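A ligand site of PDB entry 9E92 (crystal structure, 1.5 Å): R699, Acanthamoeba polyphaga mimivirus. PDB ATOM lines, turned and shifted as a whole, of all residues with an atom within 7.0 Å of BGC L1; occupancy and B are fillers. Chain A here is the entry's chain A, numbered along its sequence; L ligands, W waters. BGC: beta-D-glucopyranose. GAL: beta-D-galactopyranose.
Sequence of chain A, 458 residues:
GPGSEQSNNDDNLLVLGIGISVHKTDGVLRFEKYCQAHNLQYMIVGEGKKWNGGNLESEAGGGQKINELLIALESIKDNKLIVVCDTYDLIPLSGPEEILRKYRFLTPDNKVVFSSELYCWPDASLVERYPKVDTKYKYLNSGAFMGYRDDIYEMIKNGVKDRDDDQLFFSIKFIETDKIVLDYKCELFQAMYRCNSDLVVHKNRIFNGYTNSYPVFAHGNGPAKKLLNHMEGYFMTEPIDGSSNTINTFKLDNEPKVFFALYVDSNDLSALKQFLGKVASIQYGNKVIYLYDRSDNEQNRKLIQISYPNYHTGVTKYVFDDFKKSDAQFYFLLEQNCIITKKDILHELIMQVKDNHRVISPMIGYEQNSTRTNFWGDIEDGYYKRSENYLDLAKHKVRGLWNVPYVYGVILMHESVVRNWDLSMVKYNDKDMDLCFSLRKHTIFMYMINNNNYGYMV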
ATOM      1  N   LEU A 262      14.245 -19.786 -13.864  1.00  0.00           N
ATOM      2  CA  LEU A 262      15.422 -19.356 -14.603  1.00  0.00           C
ATOM      3  C   LEU A 262      15.270 -17.881 -14.955  1.00  0.00           C
ATOM      4  O   LEU A 262      14.286 -17.502 -15.596  1.00  0.00           O
ATOM      5  CB  LEU A 262      15.553 -20.189 -15.876  1.00  0.00           C
ATOM      6  CG  LEU A 262      15.597 -21.714 -15.751  1.00  0.00           C
ATOM      7  CD1 LEU A 262      16.014 -22.281 -17.125  1.00  0.00           C
ATOM      8  CD2 LEU A 262      16.475 -22.195 -14.681  1.00  0.00           C
ATOM      9  N   TYR A 263      16.217 -17.057 -14.551  1.00  0.00           N
ATOM     10  CA  TYR A 263      16.207 -15.626 -14.830  1.00  0.00           C
ATOM     11  C   TYR A 263      17.181 -15.379 -15.972  1.00  0.00           C
ATOM     12  O   TYR A 263      18.398 -15.556 -15.839  1.00  0.00           O
ATOM     13  CB  TYR A 263      16.505 -14.879 -13.523  1.00  0.00           C
ATOM     14  CG  TYR A 263      15.304 -14.999 -12.611  1.00  0.00           C
ATOM     15  CD1 TYR A 263      14.184 -14.214 -12.742  1.00  0.00           C
ATOM     16  CD2 TYR A 263      15.254 -16.040 -11.691  1.00  0.00           C
ATOM     17  CE1 TYR A 263      13.059 -14.405 -11.966  1.00  0.00           C
ATOM     18  CE2 TYR A 263      14.144 -16.258 -10.903  1.00  0.00           C
ATOM     19  CZ  TYR A 263      13.028 -15.450 -11.056  1.00  0.00           C
ATOM     20  OH  TYR A 263      11.890 -15.683 -10.295  1.00  0.00           O
ATOM     21  N   VAL A 264      16.605 -15.012 -17.153  1.00  0.00           N
ATOM     22  CA  VAL A 264      17.343 -15.059 -18.396  1.00  0.00           C
ATOM     23  C   VAL A 264      17.254 -13.690 -19.076  1.00  0.00           C
ATOM     24  O   VAL A 264      16.501 -12.813 -18.653  1.00  0.00           O
ATOM     25  CB  VAL A 264      16.867 -16.193 -19.330  1.00  0.00           C
ATOM     26  CG1 VAL A 264      17.034 -17.563 -18.660  1.00  0.00           C
ATOM     27  CG2 VAL A 264      15.435 -16.004 -19.840  1.00  0.00           C
ATOM     28  N   ASP A 265      18.074 -13.526 -20.127  1.00  0.00           N
ATOM     29  CA  ASP A 265      18.136 -12.296 -20.908  1.00  0.00           C
ATOM     30  C   ASP A 265      18.405 -12.643 -22.367  1.00  0.00           C
ATOM     31  O   ASP A 265      19.571 -12.851 -22.750  1.00  0.00           O
ATOM     32  CB  ASP A 265      19.191 -11.339 -20.372  1.00  0.00           C
ATOM     33  CG  ASP A 265      19.260 -10.018 -21.113  1.00  0.00           C
ATOM     34  OD1 ASP A 265      18.434  -9.828 -22.052  1.00  0.00           O
ATOM     35  OD2 ASP A 265      20.053  -9.150 -20.696  1.00  0.00           O
ATOM     36  N   ASN A 267      18.339 -10.766 -24.840  1.00  0.00           N
ATOM     37  CA  ASN A 267      19.136  -9.777 -25.524  1.00  0.00           C
ATOM     38  C   ASN A 267      20.589 -10.238 -25.704  1.00  0.00           C
ATOM     39  O   ASN A 267      21.301  -9.646 -26.502  1.00  0.00           O
ATOM     40  CB  ASN A 267      19.093  -8.422 -24.827  1.00  0.00           C
ATOM     41  CG  ASN A 267      17.712  -7.799 -24.837  1.00  0.00           C
ATOM     42  OD1 ASN A 267      16.897  -8.026 -25.770  1.00  0.00           O
ATOM     43  ND2 ASN A 267      17.392  -7.080 -23.778  1.00  0.00           N
ATOM     44  N   ASP A 268      21.033 -11.292 -24.979  1.00  0.00           N
ATOM     45  CA  ASP A 268      22.314 -11.927 -25.235  1.00  0.00           C
ATOM     46  C   ASP A 268      22.050 -13.394 -25.564  1.00  0.00           C
ATOM     47  O   ASP A 268      22.088 -14.273 -24.689  1.00  0.00           O
ATOM     48  CB  ASP A 268      23.276 -11.797 -24.053  1.00  0.00           C
ATOM     49  CG  ASP A 268      24.691 -12.266 -24.309  1.00  0.00           C
ATOM     50  OD1 ASP A 268      24.921 -12.975 -25.319  1.00  0.00           O
ATOM     51  OD2 ASP A 268      25.520 -11.989 -23.432  1.00  0.00           O
ATOM     52  N   TYR A 292      11.972 -16.647 -17.005  1.00  0.00           N
ATOM     53  CA  TYR A 292      11.596 -15.276 -16.732  1.00  0.00           C
ATOM     54  C   TYR A 292      12.626 -14.369 -17.419  1.00  0.00           C
ATOM     55  O   TYR A 292      13.754 -14.207 -16.948  1.00  0.00           O
ATOM     56  CB  TYR A 292      11.519 -15.058 -15.214  1.00  0.00           C
ATOM     57  CG  TYR A 292      10.491 -15.906 -14.502  1.00  0.00           C
ATOM     58  CD1 TYR A 292       9.132 -15.676 -14.672  1.00  0.00           C
ATOM     59  CD2 TYR A 292      10.853 -16.928 -13.626  1.00  0.00           C
ATOM     60  CE1 TYR A 292       8.187 -16.437 -14.037  1.00  0.00           C
ATOM     61  CE2 TYR A 292       9.909 -17.705 -12.982  1.00  0.00           C
ATOM     62  CZ  TYR A 292       8.557 -17.447 -13.161  1.00  0.00           C
ATOM     63  OH  TYR A 292       7.610 -18.172 -12.546  1.00  0.00           O
ATOM     64  N   ARG A 294      14.177 -10.912 -19.036  1.00  0.00           N
ATOM     65  CA  ARG A 294      14.116  -9.483 -18.831  1.00  0.00           C
ATOM     66  C   ARG A 294      13.936  -8.735 -20.144  1.00  0.00           C
ATOM     67  O   ARG A 294      13.611  -7.538 -20.093  1.00  0.00           O
ATOM     68  CB  ARG A 294      15.336  -8.943 -18.071  1.00  0.00           C
ATOM     69  CG  ARG A 294      16.674  -9.066 -18.732  1.00  0.00           C
ATOM     70  CD  ARG A 294      17.807  -8.500 -17.874  1.00  0.00           C
ATOM     71  NE  ARG A 294      17.588  -7.080 -17.485  1.00  0.00           N
ATOM     72  CZ  ARG A 294      17.096  -6.637 -16.330  1.00  0.00           C
ATOM     73  NH1 ARG A 294      16.791  -7.451 -15.349  1.00  0.00           N
ATOM     74  NH2 ARG A 294      16.986  -5.319 -16.117  1.00  0.00           N
ATOM     75  N   VAL A 315      10.346  -9.406 -17.495  1.00  0.00           N
ATOM     76  CA  VAL A 315      10.401  -9.656 -16.072  1.00  0.00           C
ATOM     77  C   VAL A 315      11.724  -9.146 -15.502  1.00  0.00           C
ATOM     78  O   VAL A 315      12.789  -9.560 -15.961  1.00  0.00           O
ATOM     79  CB  VAL A 315      10.254 -11.160 -15.788  1.00  0.00           C
ATOM     80  CG1 VAL A 315      10.365 -11.447 -14.292  1.00  0.00           C
ATOM     81  CG2 VAL A 315       8.956 -11.679 -16.376  1.00  0.00           C
ATOM     82  N   TYR A 318      12.272 -11.035  -9.089  1.00  0.00           N
ATOM     83  CA  TYR A 318      12.044 -12.424  -8.817  1.00  0.00           C
ATOM     84  C   TYR A 318      10.563 -12.662  -8.557  1.00  0.00           C
ATOM     85  O   TYR A 318       9.893 -11.881  -7.877  1.00  0.00           O
ATOM     86  CB  TYR A 318      12.973 -12.845  -7.660  1.00  0.00           C
ATOM     87  CG  TYR A 318      14.480 -12.839  -7.930  1.00  0.00           C
ATOM     88  CD1 TYR A 318      15.038 -13.140  -9.163  1.00  0.00           C
ATOM     89  CD2 TYR A 318      15.377 -12.546  -6.905  1.00  0.00           C
ATOM     90  CE1 TYR A 318      16.404 -13.174  -9.369  1.00  0.00           C
ATOM     91  CE2 TYR A 318      16.745 -12.539  -7.117  1.00  0.00           C
ATOM     92  CZ  TYR A 318      17.280 -12.842  -8.352  1.00  0.00           C
ATOM     93  OH  TYR A 318      18.613 -12.828  -8.592  1.00  0.00           O
ATOM     94  N   LEU A 334      17.936 -19.792 -10.574  1.00  0.00           N
ATOM     95  CA  LEU A 334      19.160 -19.865 -11.384  1.00  0.00           C
ATOM     96  C   LEU A 334      19.221 -18.627 -12.277  1.00  0.00           C
ATOM     97  O   LEU A 334      18.320 -18.409 -13.096  1.00  0.00           O
ATOM     98  CB  LEU A 334      19.208 -21.116 -12.265  1.00  0.00           C
ATOM     99  CG  LEU A 334      19.214 -22.470 -11.572  1.00  0.00           C
ATOM    100  CD1 LEU A 334      18.941 -23.607 -12.571  1.00  0.00           C
ATOM    101  CD2 LEU A 334      20.569 -22.657 -10.946  1.00  0.00           C
ATOM    102  N   GLU A 335      20.311 -17.853 -12.144  1.00  0.00           N
ATOM    103  CA  GLU A 335      20.596 -16.724 -13.005  1.00  0.00           C
ATOM    104  C   GLU A 335      21.464 -17.159 -14.198  1.00  0.00           C
ATOM    105  O   GLU A 335      22.362 -17.974 -14.079  1.00  0.00           O
ATOM    106  CB  GLU A 335      21.361 -15.618 -12.275  1.00  0.00           C
ATOM    107  CG  GLU A 335      20.507 -14.802 -11.305  1.00  0.00           C
ATOM    108  CD  GLU A 335      19.872 -13.574 -11.923  1.00  0.00           C
ATOM    109  OE1 GLU A 335      20.007 -13.408 -13.139  1.00  0.00           O
ATOM    110  OE2 GLU A 335      19.216 -12.810 -11.171  1.00  0.00           O
ATOM    111  N   GLN A 336      21.197 -16.522 -15.371  1.00  0.00           N
ATOM    112  CA  GLN A 336      21.870 -16.825 -16.639  1.00  0.00           C
ATOM    113  C   GLN A 336      23.382 -16.776 -16.620  1.00  0.00           C
ATOM    114  O   GLN A 336      24.021 -17.546 -17.382  1.00  0.00           O
ATOM    115  CB  GLN A 336      21.340 -15.863 -17.714  1.00  0.00           C
ATOM    116  CG  GLN A 336      21.978 -15.981 -19.101  1.00  0.00           C
ATOM    117  CD  GLN A 336      21.122 -15.301 -20.163  1.00  0.00           C
ATOM    118  OE1 GLN A 336      19.949 -15.652 -20.370  1.00  0.00           O
ATOM    119  NE2 GLN A 336      21.686 -14.300 -20.823  1.00  0.00           N
ATOM    120  N   ASN A 337      24.012 -15.903 -15.803  1.00  0.00           N
ATOM    121  CA  ASN A 337      25.480 -15.874 -15.712  1.00  0.00           C
ATOM    122  C   ASN A 337      26.095 -16.930 -14.755  1.00  0.00           C
ATOM    123  O   ASN A 337      27.328 -16.919 -14.572  1.00  0.00           O
ATOM    124  CB  ASN A 337      26.023 -14.502 -15.332  1.00  0.00           C
ATOM    125  CG  ASN A 337      25.736 -14.058 -13.922  1.00  0.00           C
ATOM    126  OD1 ASN A 337      24.707 -14.393 -13.337  1.00  0.00           O
ATOM    127  ND2 ASN A 337      26.590 -13.220 -13.378  1.00  0.00           N
ATOM    128  N   CYS A 338      25.292 -17.865 -14.223  1.00  0.00           N
ATOM    129  CA  CYS A 338      25.772 -18.933 -13.317  1.00  0.00           C
ATOM    130  C   CYS A 338      25.761 -20.278 -14.073  1.00  0.00           C
ATOM    131  O   CYS A 338      24.695 -20.746 -14.463  1.00  0.00           O
ATOM    132  CB  CYS A 338      24.916 -18.984 -12.056  1.00  0.00           C
ATOM    133  SG  CYS A 338      25.051 -17.455 -11.077  1.00  0.00           S
ATOM    134  N   TYR A 366      34.013 -16.555 -10.321  1.00  0.00           N
ATOM    135  CA  TYR A 366      34.202 -16.154 -11.697  1.00  0.00           C
ATOM    136  C   TYR A 366      35.253 -17.032 -12.358  1.00  0.00           C
ATOM    137  O   TYR A 366      36.285 -17.401 -11.767  1.00  0.00           O
ATOM    138  CB  TYR A 366      34.679 -14.702 -11.834  1.00  0.00           C
ATOM    139  CG  TYR A 366      33.481 -13.783 -11.755  1.00  0.00           C
ATOM    140  CD1 TYR A 366      32.684 -13.649 -12.884  1.00  0.00           C
ATOM    141  CD2 TYR A 366      33.112 -13.097 -10.607  1.00  0.00           C
ATOM    142  CE1 TYR A 366      31.548 -12.875 -12.848  1.00  0.00           C
ATOM    143  CE2 TYR A 366      31.985 -12.288 -10.568  1.00  0.00           C
ATOM    144  CZ  TYR A 366      31.206 -12.182 -11.710  1.00  0.00           C
ATOM    145  OH  TYR A 366      30.098 -11.387 -11.784  1.00  0.00           O
ATOM    146  N   TYR A 408      23.907 -15.354  -4.045  1.00  0.00           N
ATOM    147  CA  TYR A 408      23.437 -14.966  -5.387  1.00  0.00           C
ATOM    148  C   TYR A 408      23.337 -16.141  -6.347  1.00  0.00           C
ATOM    149  O   TYR A 408      24.244 -16.991  -6.418  1.00  0.00           O
ATOM    150  CB  TYR A 408      24.423 -13.959  -5.969  1.00  0.00           C
ATOM    151  CG  TYR A 408      24.163 -13.682  -7.449  1.00  0.00           C
ATOM    152  CD1 TYR A 408      23.093 -12.890  -7.868  1.00  0.00           C
ATOM    153  CD2 TYR A 408      25.008 -14.201  -8.416  1.00  0.00           C
ATOM    154  CE1 TYR A 408      22.853 -12.685  -9.230  1.00  0.00           C
ATOM    155  CE2 TYR A 408      24.782 -13.996  -9.781  1.00  0.00           C
ATOM    156  CZ  TYR A 408      23.691 -13.242 -10.183  1.00  0.00           C
ATOM    157  OH  TYR A 408      23.416 -13.004 -11.546  1.00  0.00           O
ATOM    158  N   LYS A 431      17.153  -6.806  -7.272  1.00  0.00           N
ATOM    159  CA  LYS A 431      16.436  -8.050  -6.962  1.00  0.00           C
ATOM    160  C   LYS A 431      17.283  -8.948  -6.049  1.00  0.00           C
ATOM    161  O   LYS A 431      16.734  -9.555  -5.125  1.00  0.00           O
ATOM    162  CB  LYS A 431      15.862  -8.744  -8.190  1.00  0.00           C
ATOM    163  CG  LYS A 431      16.810  -9.198  -9.235  1.00  0.00           C
ATOM    164  CD  LYS A 431      16.037  -9.663 -10.484  1.00  0.00           C
ATOM    165  CE  LYS A 431      16.926 -10.264 -11.523  1.00  0.00           C
ATOM    166  NZ  LYS A 431      17.773  -9.231 -12.087  1.00  0.00           N
ATOM    167  N   VAL A 458      30.128 -16.258 -15.197  1.00  0.00           N
ATOM    168  CA  VAL A 458      30.691 -15.554 -16.362  1.00  0.00           C
ATOM    169  C   VAL A 458      30.325 -14.064 -16.355  1.00  0.00           C
ATOM    170  O   VAL A 458      29.330 -13.652 -15.697  1.00  0.00           O
ATOM    171  CB  VAL A 458      30.262 -16.245 -17.659  1.00  0.00           C
ATOM    172  CG1 VAL A 458      30.776 -17.690 -17.702  1.00  0.00           C
ATOM    173  CG2 VAL A 458      28.769 -16.224 -17.887  1.00  0.00           C
ATOM    174  OXT VAL A 458      31.064 -13.292 -17.012  1.00  0.00           O
HETATM  175  C2  BGC L   1      22.937 -10.270 -17.080  1.00  0.00           C
HETATM  176  C3  BGC L   1      23.125 -11.619 -16.352  1.00  0.00           C
HETATM  177  C4  BGC L   1      21.853 -12.036 -15.622  1.00  0.00           C
HETATM  178  C5  BGC L   1      20.674 -11.965 -16.582  1.00  0.00           C
HETATM  179  C6  BGC L   1      19.332 -12.301 -15.970  1.00  0.00           C
HETATM  180  C1  BGC L   1      21.693 -10.307 -17.939  1.00  0.00           C
HETATM  181  O1  BGC L   1      21.473  -9.096 -18.541  1.00  0.00           O
HETATM  182  O2  BGC L   1      24.067  -9.997 -17.894  1.00  0.00           O
HETATM  183  O3  BGC L   1      24.203 -11.528 -15.399  1.00  0.00           O
HETATM  184  O4  BGC L   1      21.979 -13.408 -15.181  1.00  0.00           O
HETATM  185  O5  BGC L   1      20.560 -10.611 -17.099  1.00  0.00           O
HETATM  186  O6  BGC L   1      18.970 -11.577 -14.730  1.00  0.00           O
HETATM  187  C1  GAL L   2      29.227 -10.843  -8.964  1.00  0.00           C
HETATM  188  C2  GAL L   2      29.498 -11.043  -7.489  1.00  0.00           C
HETATM  189  C3  GAL L   2      28.423 -11.937  -6.880  1.00  0.00           C
HETATM  190  C4  GAL L   2      27.015 -11.437  -7.197  1.00  0.00           C
HETATM  191  C5  GAL L   2      26.898 -11.240  -8.732  1.00  0.00           C
HETATM  192  C6  GAL L   2      25.622 -10.635  -9.246  1.00  0.00           C
HETATM  193  O1  GAL L   2      30.056  -9.867  -9.525  1.00  0.00           O
HETATM  194  O2  GAL L   2      30.807 -11.571  -7.257  1.00  0.00           O
HETATM  195  O3  GAL L   2      28.599 -11.987  -5.457  1.00  0.00           O
HETATM  196  O4  GAL L   2      26.759 -10.210  -6.509  1.00  0.00           O
HETATM  197  O5  GAL L   2      27.907 -10.332  -9.101  1.00  0.00           O
HETATM  198  O6  GAL L   2      25.646 -10.687 -10.686  1.00  0.00           O
HETATM  199  O   HOH W   1      16.628 -10.346 -14.960  1.00  0.00           O
HETATM  200  O   HOH W   2      24.073 -12.689 -19.998  1.00  0.00           O
HETATM  201  O   HOH W   3      19.723  -8.978 -14.206  1.00  0.00           O
HETATM  202  O   HOH W   4      26.703 -11.013 -16.623  1.00  0.00           O
HETATM  203  O   HOH W   5      23.533 -10.773 -12.754  1.00  0.00           O
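Water W1 lies within hydrogen-bond range of O6 of BGC L1, NH1 of Arg 294 and NZ of Lys 431. Water W3 lies within hydrogen-bond range of O6 of BGC L1, NZ of Lys 431 and NH1 of Arg 294. Water W5 lies within hydrogen-bond range of the side-chain hydroxyl (OH) of Tyr 408 (2.5 Å), an oxygen (O3) of BGC L1 (2.8 Å) and an oxygen (O6) of GAL L2 (3.0 Å). Water W2 bridges NE2 of Gln 336 and O2 of BGC L1.
Tyr 263 touches BGC L1. Val 264 touches BGC L1. CD of Arg 294 touches O5 of BGC L1, 3.6 Å away. Tyr 408 touches BGC L1 (OH to O4, 3.9 Å). NZ of Lys 431 touches O6 of BGC L1 (3.7 Å).
The backbone carbonyl oxygen (O) of Leu 334 is in hydrogen-bond range of the backbone NH (N) of Tyr 263. O of Asn 337 is in hydrogen-bond range of N of Val 458 (2.9 Å). The backbone carbonyl oxygen of Tyr 292 sits at hydrogen-bond distance from the backbone NH of Val 264. N of Asp 265 sits at hydrogen-bond distance from OE1 of Gln 336 (2.8 Å). OD1 of Asp 265 is in hydrogen-bond range of N of Asn 267, at 2.9 Å. OD1 of Asn 337 sits at hydrogen-bond distance from OH of Tyr 408, at 2.6 Å. The backbone NH of Gln 336 lies within hydrogen-bond range of the backbone carbonyl oxygen of Tyr 263, 3.0 Å away. OE2 of Glu 335 is in salt-bridge range of NZ of Lys 431 (3.97 Å).
OD1 of Asn 337 lies within hydrogen-bond range of O4 of BGC L1 (3.4 Å). O4 of BGC L1 sits at hydrogen-bond distance from N of Asn 337, 3.3 Å away. The side-chain hydroxyl of Tyr 408 sits close to an oxygen (O6) of GAL L2 (3.3 Å). An oxygen (O1) of BGC L1 lies within hydrogen-bond range of the side-chain carboxylate (OD2) of Asp 265 (2.6 Å). N of Gln 336 lies within hydrogen-bond range of O4 of BGC L1, 3.2 Å away. OH of Tyr 366 sits at hydrogen-bond distance from O1 of GAL L2 (2.7 Å). The side-chain carboxylate of Glu 335 sits at hydrogen-bond distance from an oxygen (O6) of BGC L1 (2.6 Å).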
